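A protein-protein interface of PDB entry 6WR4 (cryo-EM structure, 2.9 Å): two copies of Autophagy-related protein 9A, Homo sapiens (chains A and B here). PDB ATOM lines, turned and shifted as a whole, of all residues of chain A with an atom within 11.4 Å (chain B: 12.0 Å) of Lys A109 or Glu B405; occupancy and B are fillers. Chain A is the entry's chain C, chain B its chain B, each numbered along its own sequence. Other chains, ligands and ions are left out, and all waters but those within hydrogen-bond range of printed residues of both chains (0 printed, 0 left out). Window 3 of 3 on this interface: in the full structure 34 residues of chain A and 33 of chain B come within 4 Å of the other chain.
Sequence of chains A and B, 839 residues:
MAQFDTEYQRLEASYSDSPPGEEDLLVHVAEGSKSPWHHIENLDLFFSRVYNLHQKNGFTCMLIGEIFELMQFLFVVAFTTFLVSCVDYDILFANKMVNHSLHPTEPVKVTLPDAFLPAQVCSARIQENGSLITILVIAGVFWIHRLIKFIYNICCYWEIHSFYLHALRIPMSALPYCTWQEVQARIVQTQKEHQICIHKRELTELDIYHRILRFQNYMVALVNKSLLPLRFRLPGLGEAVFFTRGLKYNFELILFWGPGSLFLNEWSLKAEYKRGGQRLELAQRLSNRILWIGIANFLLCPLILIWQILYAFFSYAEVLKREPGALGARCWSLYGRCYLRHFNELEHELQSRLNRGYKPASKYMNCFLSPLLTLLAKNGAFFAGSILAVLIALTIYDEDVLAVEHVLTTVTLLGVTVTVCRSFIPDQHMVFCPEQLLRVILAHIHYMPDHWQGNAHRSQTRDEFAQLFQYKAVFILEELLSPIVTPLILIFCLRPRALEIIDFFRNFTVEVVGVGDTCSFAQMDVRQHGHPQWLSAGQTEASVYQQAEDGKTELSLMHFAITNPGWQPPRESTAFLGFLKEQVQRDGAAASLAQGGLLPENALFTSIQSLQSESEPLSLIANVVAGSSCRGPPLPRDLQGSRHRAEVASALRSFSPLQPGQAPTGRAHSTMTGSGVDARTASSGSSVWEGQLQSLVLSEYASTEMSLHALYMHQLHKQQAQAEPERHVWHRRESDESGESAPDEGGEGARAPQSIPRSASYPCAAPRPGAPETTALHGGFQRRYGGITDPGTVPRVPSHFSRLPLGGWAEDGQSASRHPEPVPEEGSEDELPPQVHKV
Of the printed residues of chain B, Lys A109 touches Ala B403 (3.1 Å) and Glu B405 (3.4 Å).
Of chain A, only Lys A109 (3.4 Å), Val A110 (3.3 Å), Thr A111 (3.6 Å) and Leu A112 (3.9 Å) come within 4 Å of Glu B405.
Of chain B, only Val B404 (3.5 Å) and Glu B405 (3.3 Å) come within 4 Å of Val A110.
Of the printed residues of chain A, Ala B403 touches Lys A109 (3.1 Å).
Of chain A, only Leu A92 (3.9 Å), Val A110 (3.5 Å) and Thr A111 (3.7 Å) come within 4 Å of Val B404.
No residue of chain A comes within 4 Å of His B406.
Of the printed residues of chain B, Leu A112 touches Glu B405.
Of the printed residues of chain A, Val B401 touches Leu A92 and Phe A93.
Of the printed residues of chain A, Leu B394 touches Leu A92 and Phe A93.
Of the printed residues of chain B, Leu A92 touches Leu B394 (3.9 Å), Asp B400 (3.7 Å), Val B401 (3.6 Å) and Val B404 (3.9 Å).
Of the printed residues of chain B, Phe A93 touches Leu B394 (3.7 Å), Asp B400 (3.1 Å) and Val B401 (3.5 Å).
Leu B402 touches none of the printed residues of chain A.
The nearest printed residue of chain B that does not touch Phe A93 is Glu B399 (6.3 Å).
Positions printed for both chains: 93 and 94.
Among the printed residues, merely in contact across the chains: Lys A109 with Glu B405 (3.4 Å), Val A110 with Val B404 (3.5 Å), Phe A93 with Val B401 (3.5 Å), Thr A111 with Glu B405 (3.6 Å), Leu A92 with Val B401 (3.6 Å), Phe A93 with Leu B394 (3.7 Å), Leu A92 with Asp B400 (3.7 Å), Thr A111 with Val B404 (3.7 Å), Leu A92 with Leu B394 (3.9 Å), Leu A92 with Val B404 (3.9 Å) and Leu A112 with Glu B405 (3.9 Å).
O of Ala B403 lies within hydrogen-bond range of NZ of Lys A109.
The side-chain carboxylate of Asp B400 sits close to the backbone carbonyl oxygen of Phe A93.
O of Val A110 lies within hydrogen-bond range of N of Glu B405, 3.3 Å away.
Of the 20 printed residues of chain B, 6 touch a printed residue of chain A.
Printed residues of chain B that touch a printed residue of chain A: Leu B394, Asp B400, Val B401, Ala B403, Val B404 and Glu B405.
Printed residues of chain A that touch a printed residue of chain B: Leu A92, Phe A93, Lys A109, Val A110, Thr A111 and Leu A112.
Hydrophobic or aromatic side chains of chain A that line the printed part of chain B: Leu A92, Phe A93 and Val A110.
Among the printed residues, no Asp or Glu carboxylate lies within 4 Å of a Lys or Arg side-chain nitrogen of the other chain.
OG1 of Thr A111 lies close to N of Asp A114.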
ATOM      1  N   ILE A  91       9.193  20.607 -31.148  1.00  0.00           N
ATOM      2  CA  ILE A  91       9.324  19.629 -30.077  1.00  0.00           C
ATOM      3  C   ILE A  91      10.742  19.064 -30.055  1.00  0.00           C
ATOM      4  O   ILE A  91      11.311  18.798 -28.989  1.00  0.00           O
ATOM      5  CB  ILE A  91       8.252  18.535 -30.244  1.00  0.00           C
ATOM      6  CG1 ILE A  91       6.866  19.161 -30.107  1.00  0.00           C
ATOM      7  CG2 ILE A  91       8.400  17.428 -29.226  1.00  0.00           C
ATOM      8  CD1 ILE A  91       5.738  18.226 -30.440  1.00  0.00           C
ATOM      9  N   LEU A  92      11.361  18.941 -31.229  1.00  0.00           N
ATOM     10  CA  LEU A  92      12.676  18.314 -31.309  1.00  0.00           C
ATOM     11  C   LEU A  92      13.783  19.271 -30.876  1.00  0.00           C
ATOM     12  O   LEU A  92      14.804  18.845 -30.326  1.00  0.00           O
ATOM     13  CB  LEU A  92      12.913  17.804 -32.727  1.00  0.00           C
ATOM     14  CG  LEU A  92      14.157  16.964 -32.980  1.00  0.00           C
ATOM     15  CD1 LEU A  92      14.114  15.720 -32.146  1.00  0.00           C
ATOM     16  CD2 LEU A  92      14.228  16.600 -34.428  1.00  0.00           C
ATOM     17  N   PHE A  93      13.602  20.576 -31.107  1.00  0.00           N
ATOM     18  CA  PHE A  93      14.632  21.544 -30.726  1.00  0.00           C
ATOM     19  C   PHE A  93      14.417  22.072 -29.316  1.00  0.00           C
ATOM     20  O   PHE A  93      15.284  21.925 -28.450  1.00  0.00           O
ATOM     21  CB  PHE A  93      14.660  22.717 -31.706  1.00  0.00           C
ATOM     22  CG  PHE A  93      15.248  22.387 -33.041  1.00  0.00           C
ATOM     23  CD1 PHE A  93      16.082  21.303 -33.199  1.00  0.00           C
ATOM     24  CD2 PHE A  93      14.945  23.157 -34.147  1.00  0.00           C
ATOM     25  CE1 PHE A  93      16.621  21.001 -34.431  1.00  0.00           C
ATOM     26  CE2 PHE A  93      15.476  22.851 -35.376  1.00  0.00           C
ATOM     27  CZ  PHE A  93      16.316  21.770 -35.516  1.00  0.00           C
ATOM     28  N   ALA A  94      13.271  22.699 -29.070  1.00  0.00           N
ATOM     29  CA  ALA A  94      13.045  23.421 -27.831  1.00  0.00           C
ATOM     30  C   ALA A  94      12.178  22.678 -26.829  1.00  0.00           C
ATOM     31  O   ALA A  94      12.518  22.662 -25.644  1.00  0.00           O
ATOM     32  CB  ALA A  94      12.394  24.782 -28.123  1.00  0.00           C
ATOM     33  N   ASN A  95      11.090  22.055 -27.271  1.00  0.00           N
ATOM     34  CA  ASN A  95      10.085  21.517 -26.358  1.00  0.00           C
ATOM     35  C   ASN A  95      10.222  20.007 -26.167  1.00  0.00           C
ATOM     36  O   ASN A  95       9.306  19.348 -25.676  1.00  0.00           O
ATOM     37  CB  ASN A  95       8.685  21.854 -26.871  1.00  0.00           C
ATOM     38  CG  ASN A  95       8.395  23.341 -26.834  1.00  0.00           C
ATOM     39  OD1 ASN A  95       8.715  24.022 -25.863  1.00  0.00           O
ATOM     40  ND2 ASN A  95       7.796  23.854 -27.900  1.00  0.00           N
ATOM     41  N   LYS A 109      11.259  14.701 -20.063  1.00  0.00           N
ATOM     42  CA  LYS A 109      12.021  13.970 -21.068  1.00  0.00           C
ATOM     43  C   LYS A 109      11.185  13.726 -22.317  1.00  0.00           C
ATOM     44  O   LYS A 109      10.073  13.205 -22.238  1.00  0.00           O
ATOM     45  CB  LYS A 109      12.513  12.639 -20.503  1.00  0.00           C
ATOM     46  CG  LYS A 109      13.381  11.848 -21.459  1.00  0.00           C
ATOM     47  CD  LYS A 109      14.735  12.500 -21.624  1.00  0.00           C
ATOM     48  CE  LYS A 109      15.649  11.650 -22.477  1.00  0.00           C
ATOM     49  NZ  LYS A 109      16.973  12.299 -22.674  1.00  0.00           N
ATOM     50  N   VAL A 110      11.731  14.107 -23.468  1.00  0.00           N
ATOM     51  CA  VAL A 110      11.082  13.937 -24.764  1.00  0.00           C
ATOM     52  C   VAL A 110      11.682  12.715 -25.440  1.00  0.00           C
ATOM     53  O   VAL A 110      12.844  12.370 -25.198  1.00  0.00           O
ATOM     54  CB  VAL A 110      11.225  15.186 -25.647  1.00  0.00           C
ATOM     55  CG1 VAL A 110      10.071  15.278 -26.625  1.00  0.00           C
ATOM     56  CG2 VAL A 110      11.262  16.435 -24.792  1.00  0.00           C
ATOM     57  N   THR A 111      10.879  12.048 -26.261  1.00  0.00           N
ATOM     58  CA  THR A 111      11.305  10.891 -27.028  1.00  0.00           C
ATOM     59  C   THR A 111      11.468  11.261 -28.497  1.00  0.00           C
ATOM     60  O   THR A 111      10.929  12.266 -28.962  1.00  0.00           O
ATOM     61  CB  THR A 111      10.297   9.753 -26.878  1.00  0.00           C
ATOM     62  OG1 THR A 111       9.046  10.145 -27.450  1.00  0.00           O
ATOM     63  CG2 THR A 111      10.077   9.447 -25.407  1.00  0.00           C
ATOM     64  N   LEU A 112      12.229  10.447 -29.226  1.00  0.00           N
ATOM     65  CA  LEU A 112      12.408  10.679 -30.661  1.00  0.00           C
ATOM     66  C   LEU A 112      11.157  10.413 -31.503  1.00  0.00           C
ATOM     67  O   LEU A 112      10.931  11.167 -32.462  1.00  0.00           O
ATOM     68  CB  LEU A 112      13.626   9.881 -31.159  1.00  0.00           C
ATOM     69  CG  LEU A 112      14.053  10.011 -32.622  1.00  0.00           C
ATOM     70  CD1 LEU A 112      14.369  11.447 -32.957  1.00  0.00           C
ATOM     71  CD2 LEU A 112      15.265   9.143 -32.887  1.00  0.00           C
ATOM     72  N   PRO A 113      10.304   9.409 -31.224  1.00  0.00           N
ATOM     73  CA  PRO A 113       9.000   9.377 -31.912  1.00  0.00           C
ATOM     74  C   PRO A 113       7.975  10.386 -31.410  1.00  0.00           C
ATOM     75  O   PRO A 113       6.836  10.351 -31.889  1.00  0.00           O
ATOM     76  CB  PRO A 113       8.504   7.949 -31.666  1.00  0.00           C
ATOM     77  CG  PRO A 113       9.703   7.172 -31.429  1.00  0.00           C
ATOM     78  CD  PRO A 113      10.595   8.073 -30.662  1.00  0.00           C
ATOM     79  N   ASP A 114       8.306  11.261 -30.466  1.00  0.00           N
ATOM     80  CA  ASP A 114       7.389  12.332 -30.106  1.00  0.00           C
ATOM     81  C   ASP A 114       7.424  13.465 -31.119  1.00  0.00           C
ATOM     82  O   ASP A 114       6.439  14.197 -31.255  1.00  0.00           O
ATOM     83  CB  ASP A 114       7.725  12.878 -28.713  1.00  0.00           C
ATOM     84  CG  ASP A 114       6.570  13.635 -28.074  1.00  0.00           C
ATOM     85  OD1 ASP A 114       5.467  13.677 -28.658  1.00  0.00           O
ATOM     86  OD2 ASP A 114       6.771  14.194 -26.975  1.00  0.00           O
ATOM     87  N   ALA A 115       8.535  13.613 -31.838  1.00  0.00           N
ATOM     88  CA  ALA A 115       8.628  14.640 -32.867  1.00  0.00           C
ATOM     89  C   ALA A 115       7.757  14.293 -34.065  1.00  0.00           C
ATOM     90  O   ALA A 115       7.152  15.176 -34.681  1.00  0.00           O
ATOM     91  CB  ALA A 115      10.085  14.813 -33.290  1.00  0.00           C
ATOM     92  N   PHE A 116       7.668  13.002 -34.390  1.00  0.00           N
ATOM     93  CA  PHE A 116       7.023  12.540 -35.614  1.00  0.00           C
ATOM     94  C   PHE A 116       5.514  12.749 -35.547  1.00  0.00           C
ATOM     95  O   PHE A 116       4.898  12.662 -34.484  1.00  0.00           O
ATOM     96  CB  PHE A 116       7.316  11.056 -35.846  1.00  0.00           C
ATOM     97  CG  PHE A 116       8.764  10.739 -36.135  1.00  0.00           C
ATOM     98  CD1 PHE A 116       9.656  11.720 -36.531  1.00  0.00           C
ATOM     99  CD2 PHE A 116       9.226   9.443 -36.005  1.00  0.00           C
ATOM    100  CE1 PHE A 116      10.980  11.411 -36.788  1.00  0.00           C
ATOM    101  CE2 PHE A 116      10.547   9.131 -36.262  1.00  0.00           C
ATOM    102  CZ  PHE A 116      11.422  10.116 -36.655  1.00  0.00           C
ATOM    103  N   PHE B  93      21.526   3.727 -13.554  1.00  0.00           N
ATOM    104  CA  PHE B  93      20.732   3.965 -14.762  1.00  0.00           C
ATOM    105  C   PHE B  93      19.697   5.059 -14.549  1.00  0.00           C
ATOM    106  O   PHE B  93      19.703   6.075 -15.249  1.00  0.00           O
ATOM    107  CB  PHE B  93      20.027   2.683 -15.206  1.00  0.00           C
ATOM    108  CG  PHE B  93      20.936   1.666 -15.820  1.00  0.00           C
ATOM    109  CD1 PHE B  93      22.156   2.030 -16.344  1.00  0.00           C
ATOM    110  CD2 PHE B  93      20.573   0.334 -15.853  1.00  0.00           C
ATOM    111  CE1 PHE B  93      22.991   1.091 -16.908  1.00  0.00           C
ATOM    112  CE2 PHE B  93      21.408  -0.604 -16.408  1.00  0.00           C
ATOM    113  CZ  PHE B  93      22.621  -0.222 -16.936  1.00  0.00           C
ATOM    114  N   ALA B  94      18.792   4.863 -13.595  1.00  0.00           N
ATOM    115  CA  ALA B  94      17.640   5.734 -13.442  1.00  0.00           C
ATOM    116  C   ALA B  94      17.766   6.735 -12.308  1.00  0.00           C
ATOM    117  O   ALA B  94      17.425   7.905 -12.504  1.00  0.00           O
ATOM    118  CB  ALA B  94      16.371   4.898 -13.216  1.00  0.00           C
ATOM    119  N   LEU B 391      21.187  13.465 -38.873  1.00  0.00           N
ATOM    120  CA  LEU B 391      21.392  13.678 -37.444  1.00  0.00           C
ATOM    121  C   LEU B 391      22.660  14.448 -37.113  1.00  0.00           C
ATOM    122  O   LEU B 391      22.663  15.180 -36.123  1.00  0.00           O
ATOM    123  CB  LEU B 391      21.417  12.344 -36.698  1.00  0.00           C
ATOM    124  CG  LEU B 391      20.076  11.633 -36.561  1.00  0.00           C
ATOM    125  CD1 LEU B 391      20.265  10.270 -35.937  1.00  0.00           C
ATOM    126  CD2 LEU B 391      19.138  12.478 -35.736  1.00  0.00           C
ATOM    127  N   LEU B 394      21.821  17.990 -37.921  1.00  0.00           N
ATOM    128  CA  LEU B 394      20.782  18.482 -37.030  1.00  0.00           C
ATOM    129  C   LEU B 394      21.323  18.753 -35.633  1.00  0.00           C
ATOM    130  O   LEU B 394      20.725  19.540 -34.894  1.00  0.00           O
ATOM    131  CB  LEU B 394      19.648  17.468 -36.987  1.00  0.00           C
ATOM    132  CG  LEU B 394      18.257  17.750 -36.468  1.00  0.00           C
ATOM    133  CD1 LEU B 394      17.616  18.795 -37.340  1.00  0.00           C
ATOM    134  CD2 LEU B 394      17.501  16.453 -36.563  1.00  0.00           C
ATOM    135  N   THR B 395      22.429  18.108 -35.252  1.00  0.00           N
ATOM    136  CA  THR B 395      23.139  18.442 -34.024  1.00  0.00           C
ATOM    137  C   THR B 395      23.967  19.707 -34.149  1.00  0.00           C
ATOM    138  O   THR B 395      24.065  20.456 -33.178  1.00  0.00           O
ATOM    139  CB  THR B 395      24.073  17.304 -33.588  1.00  0.00           C
ATOM    140  OG1 THR B 395      24.923  16.927 -34.674  1.00  0.00           O
ATOM    141  CG2 THR B 395      23.313  16.104 -33.084  1.00  0.00           C
ATOM    142  N   GLU B 399      22.120  21.593 -31.364  1.00  0.00           N
ATOM    143  CA  GLU B 399      22.815  20.937 -30.233  1.00  0.00           C
ATOM    144  C   GLU B 399      21.902  20.659 -29.043  1.00  0.00           C
ATOM    145  O   GLU B 399      22.372  20.470 -27.923  1.00  0.00           O
ATOM    146  CB  GLU B 399      24.035  21.742 -29.761  1.00  0.00           C
ATOM    147  CG  GLU B 399      25.444  21.420 -30.313  1.00  0.00           C
ATOM    148  CD  GLU B 399      25.830  19.963 -30.619  1.00  0.00           C
ATOM    149  OE1 GLU B 399      25.299  19.002 -30.022  1.00  0.00           O
ATOM    150  OE2 GLU B 399      26.707  19.780 -31.487  1.00  0.00           O
ATOM    151  N   ASP B 400      20.597  20.647 -29.268  1.00  0.00           N
ATOM    152  CA  ASP B 400      19.655  20.189 -28.266  1.00  0.00           C
ATOM    153  C   ASP B 400      18.816  19.044 -28.815  1.00  0.00           C
ATOM    154  O   ASP B 400      17.847  18.635 -28.172  1.00  0.00           O
ATOM    155  CB  ASP B 400      18.778  21.357 -27.788  1.00  0.00           C
ATOM    156  CG  ASP B 400      18.163  21.113 -26.436  1.00  0.00           C
ATOM    157  OD1 ASP B 400      18.657  20.227 -25.715  1.00  0.00           O
ATOM    158  OD2 ASP B 400      17.208  21.833 -26.078  1.00  0.00           O
ATOM    159  N   VAL B 401      19.168  18.517 -29.987  1.00  0.00           N
ATOM    160  CA  VAL B 401      18.635  17.233 -30.427  1.00  0.00           C
ATOM    161  C   VAL B 401      19.497  16.104 -29.886  1.00  0.00           C
ATOM    162  O   VAL B 401      19.249  14.924 -30.151  1.00  0.00           O
ATOM    163  CB  VAL B 401      18.542  17.175 -31.958  1.00  0.00           C
ATOM    164  CG1 VAL B 401      17.727  18.305 -32.443  1.00  0.00           C
ATOM    165  CG2 VAL B 401      19.893  17.233 -32.562  1.00  0.00           C
ATOM    166  N   LEU B 402      20.560  16.453 -29.172  1.00  0.00           N
ATOM    167  CA  LEU B 402      21.116  15.539 -28.192  1.00  0.00           C
ATOM    168  C   LEU B 402      20.289  15.750 -26.933  1.00  0.00           C
ATOM    169  O   LEU B 402      19.636  16.788 -26.805  1.00  0.00           O
ATOM    170  CB  LEU B 402      22.603  15.799 -27.978  1.00  0.00           C
ATOM    171  CG  LEU B 402      23.450  15.569 -29.231  1.00  0.00           C
ATOM    172  CD1 LEU B 402      24.893  15.947 -28.996  1.00  0.00           C
ATOM    173  CD2 LEU B 402      23.348  14.129 -29.675  1.00  0.00           C
ATOM    174  N   ALA B 403      20.265  14.765 -26.039  1.00  0.00           N
ATOM    175  CA  ALA B 403      19.400  14.663 -24.852  1.00  0.00           C
ATOM    176  C   ALA B 403      17.916  14.633 -25.202  1.00  0.00           C
ATOM    177  O   ALA B 403      17.079  14.942 -24.347  1.00  0.00           O
ATOM    178  CB  ALA B 403      19.656  15.759 -23.808  1.00  0.00           C
ATOM    179  N   VAL B 404      17.563  14.283 -26.434  1.00  0.00           N
ATOM    180  CA  VAL B 404      16.276  13.679 -26.734  1.00  0.00           C
ATOM    181  C   VAL B 404      16.578  12.202 -26.993  1.00  0.00           C
ATOM    182  O   VAL B 404      17.671  11.849 -27.450  1.00  0.00           O
ATOM    183  CB  VAL B 404      15.547  14.402 -27.903  1.00  0.00           C
ATOM    184  CG1 VAL B 404      16.230  14.217 -29.210  1.00  0.00           C
ATOM    185  CG2 VAL B 404      14.090  14.019 -28.013  1.00  0.00           C
ATOM    186  N   GLU B 405      15.583  11.344 -26.708  1.00  0.00           N
ATOM    187  CA  GLU B 405      15.763  10.014 -26.103  1.00  0.00           C
ATOM    188  C   GLU B 405      16.884   9.132 -26.647  1.00  0.00           C
ATOM    189  O   GLU B 405      17.841   8.827 -25.930  1.00  0.00           O
ATOM    190  CB  GLU B 405      14.447   9.244 -26.209  1.00  0.00           C
ATOM    191  CG  GLU B 405      14.451   7.858 -25.586  1.00  0.00           C
ATOM    192  CD  GLU B 405      14.521   7.867 -24.076  1.00  0.00           C
ATOM    193  OE1 GLU B 405      14.071   8.853 -23.457  1.00  0.00           O
ATOM    194  OE2 GLU B 405      15.021   6.874 -23.508  1.00  0.00           O
ATOM    195  N   HIS B 406      16.791   8.701 -27.905  1.00  0.00           N
ATOM    196  CA  HIS B 406      17.739   7.694 -28.365  1.00  0.00           C
ATOM    197  C   HIS B 406      18.731   8.226 -29.382  1.00  0.00           C
ATOM    198  O   HIS B 406      19.334   7.426 -30.098  1.00  0.00           O
ATOM    199  CB  HIS B 406      17.049   6.491 -29.012  1.00  0.00           C
ATOM    200  CG  HIS B 406      16.229   5.672 -28.070  1.00  0.00           C
ATOM    201  ND1 HIS B 406      16.788   4.902 -27.074  1.00  0.00           N
ATOM    202  CD2 HIS B 406      14.896   5.450 -28.013  1.00  0.00           C
ATOM    203  CE1 HIS B 406      15.831   4.274 -26.417  1.00  0.00           C
ATOM    204  NE2 HIS B 406      14.672   4.591 -26.966  1.00  0.00           N
ATOM    205  N   VAL B 407      18.914   9.542 -29.476  1.00  0.00           N
ATOM    206  CA  VAL B 407      19.686  10.095 -30.585  1.00  0.00           C
ATOM    207  C   VAL B 407      21.173   9.829 -30.411  1.00  0.00           C
ATOM    208  O   VAL B 407      21.868   9.498 -31.382  1.00  0.00           O
ATOM    209  CB  VAL B 407      19.371  11.595 -30.737  1.00  0.00           C
ATOM    210  CG1 VAL B 407      20.298  12.260 -31.735  1.00  0.00           C
ATOM    211  CG2 VAL B 407      17.964  11.743 -31.214  1.00  0.00           C
ATOM    212  N   LEU B 408      21.671   9.892 -29.177  1.00  0.00           N
ATOM    213  CA  LEU B 408      23.111   9.786 -28.973  1.00  0.00           C
ATOM    214  C   LEU B 408      23.589   8.345 -29.126  1.00  0.00           C
ATOM    215  O   LEU B 408      24.727   8.110 -29.549  1.00  0.00           O
ATOM    216  CB  LEU B 408      23.475  10.371 -27.608  1.00  0.00           C
ATOM    217  CG  LEU B 408      24.917  10.817 -27.362  1.00  0.00           C
ATOM    218  CD1 LEU B 408      24.900  12.030 -26.462  1.00  0.00           C
ATOM    219  CD2 LEU B 408      25.754   9.731 -26.726  1.00  0.00           C
ATOM    220  N   THR B 409      22.731   7.364 -28.814  1.00  0.00           N
ATOM    221  CA  THR B 409      23.089   5.974 -29.090  1.00  0.00           C
ATOM    222  C   THR B 409      22.822   5.612 -30.539  1.00  0.00           C
ATOM    223  O   THR B 409      23.357   4.619 -31.043  1.00  0.00           O
ATOM    224  CB  THR B 409      22.344   5.008 -28.168  1.00  0.00           C
ATOM    225  OG1 THR B 409      22.815   3.677 -28.399  1.00  0.00           O
ATOM    226  CG2 THR B 409      20.855   5.047 -28.393  1.00  0.00           C
ATOM    227  N   THR B 410      21.998   6.399 -31.228  1.00  0.00           N
ATOM    228  CA  THR B 410      21.759   6.146 -32.640  1.00  0.00           C
ATOM    229  C   THR B 410      22.956   6.590 -33.465  1.00  0.00           C
ATOM    230  O   THR B 410      23.372   5.890 -34.387  1.00  0.00           O
ATOM    231  CB  THR B 410      20.486   6.859 -33.083  1.00  0.00           C
ATOM    232  OG1 THR B 410      19.423   6.493 -32.201  1.00  0.00           O
ATOM    233  CG2 THR B 410      20.091   6.433 -34.460  1.00  0.00           C
ATOM    234  N   VAL B 411      23.544   7.737 -33.118  1.00  0.00           N
ATOM    235  CA  VAL B 411      24.772   8.195 -33.766  1.00  0.00           C
ATOM    236  C   VAL B 411      25.922   7.242 -33.458  1.00  0.00           C
ATOM    237  O   VAL B 411      26.790   6.990 -34.305  1.00  0.00           O
ATOM    238  CB  VAL B 411      25.084   9.638 -33.323  1.00  0.00           C
ATOM    239  CG1 VAL B 411      26.372  10.146 -33.929  1.00  0.00           C
ATOM    240  CG2 VAL B 411      23.942  10.560 -33.688  1.00  0.00           C
ATOM    241  N   THR B 412      25.914   6.658 -32.257  1.00  0.00           N
ATOM    242  CA  THR B 412      26.958   5.720 -31.859  1.00  0.00           C
ATOM    243  C   THR B 412      26.849   4.415 -32.638  1.00  0.00           C
ATOM    244  O   THR B 412      27.853   3.888 -33.131  1.00  0.00           O
ATOM    245  CB  THR B 412      26.860   5.457 -30.357  1.00  0.00           C
ATOM    246  OG1 THR B 412      26.945   6.699 -29.652  1.00  0.00           O
ATOM    247  CG2 THR B 412      27.981   4.553 -29.893  1.00  0.00           C
ATOM    248  N   LEU B 413      25.629   3.891 -32.778  1.00  0.00           N
ATOM    249  CA  LEU B 413      25.450   2.604 -33.441  1.00  0.00           C
ATOM    250  C   LEU B 413      25.450   2.737 -34.960  1.00  0.00           C
ATOM    251  O   LEU B 413      25.885   1.819 -35.660  1.00  0.00           O
ATOM    252  CB  LEU B 413      24.166   1.941 -32.956  1.00  0.00           C
ATOM    253  CG  LEU B 413      24.199   1.429 -31.522  1.00  0.00           C
ATOM    254  CD1 LEU B 413      22.822   0.976 -31.088  1.00  0.00           C
ATOM    255  CD2 LEU B 413      25.202   0.295 -31.415  1.00  0.00           C
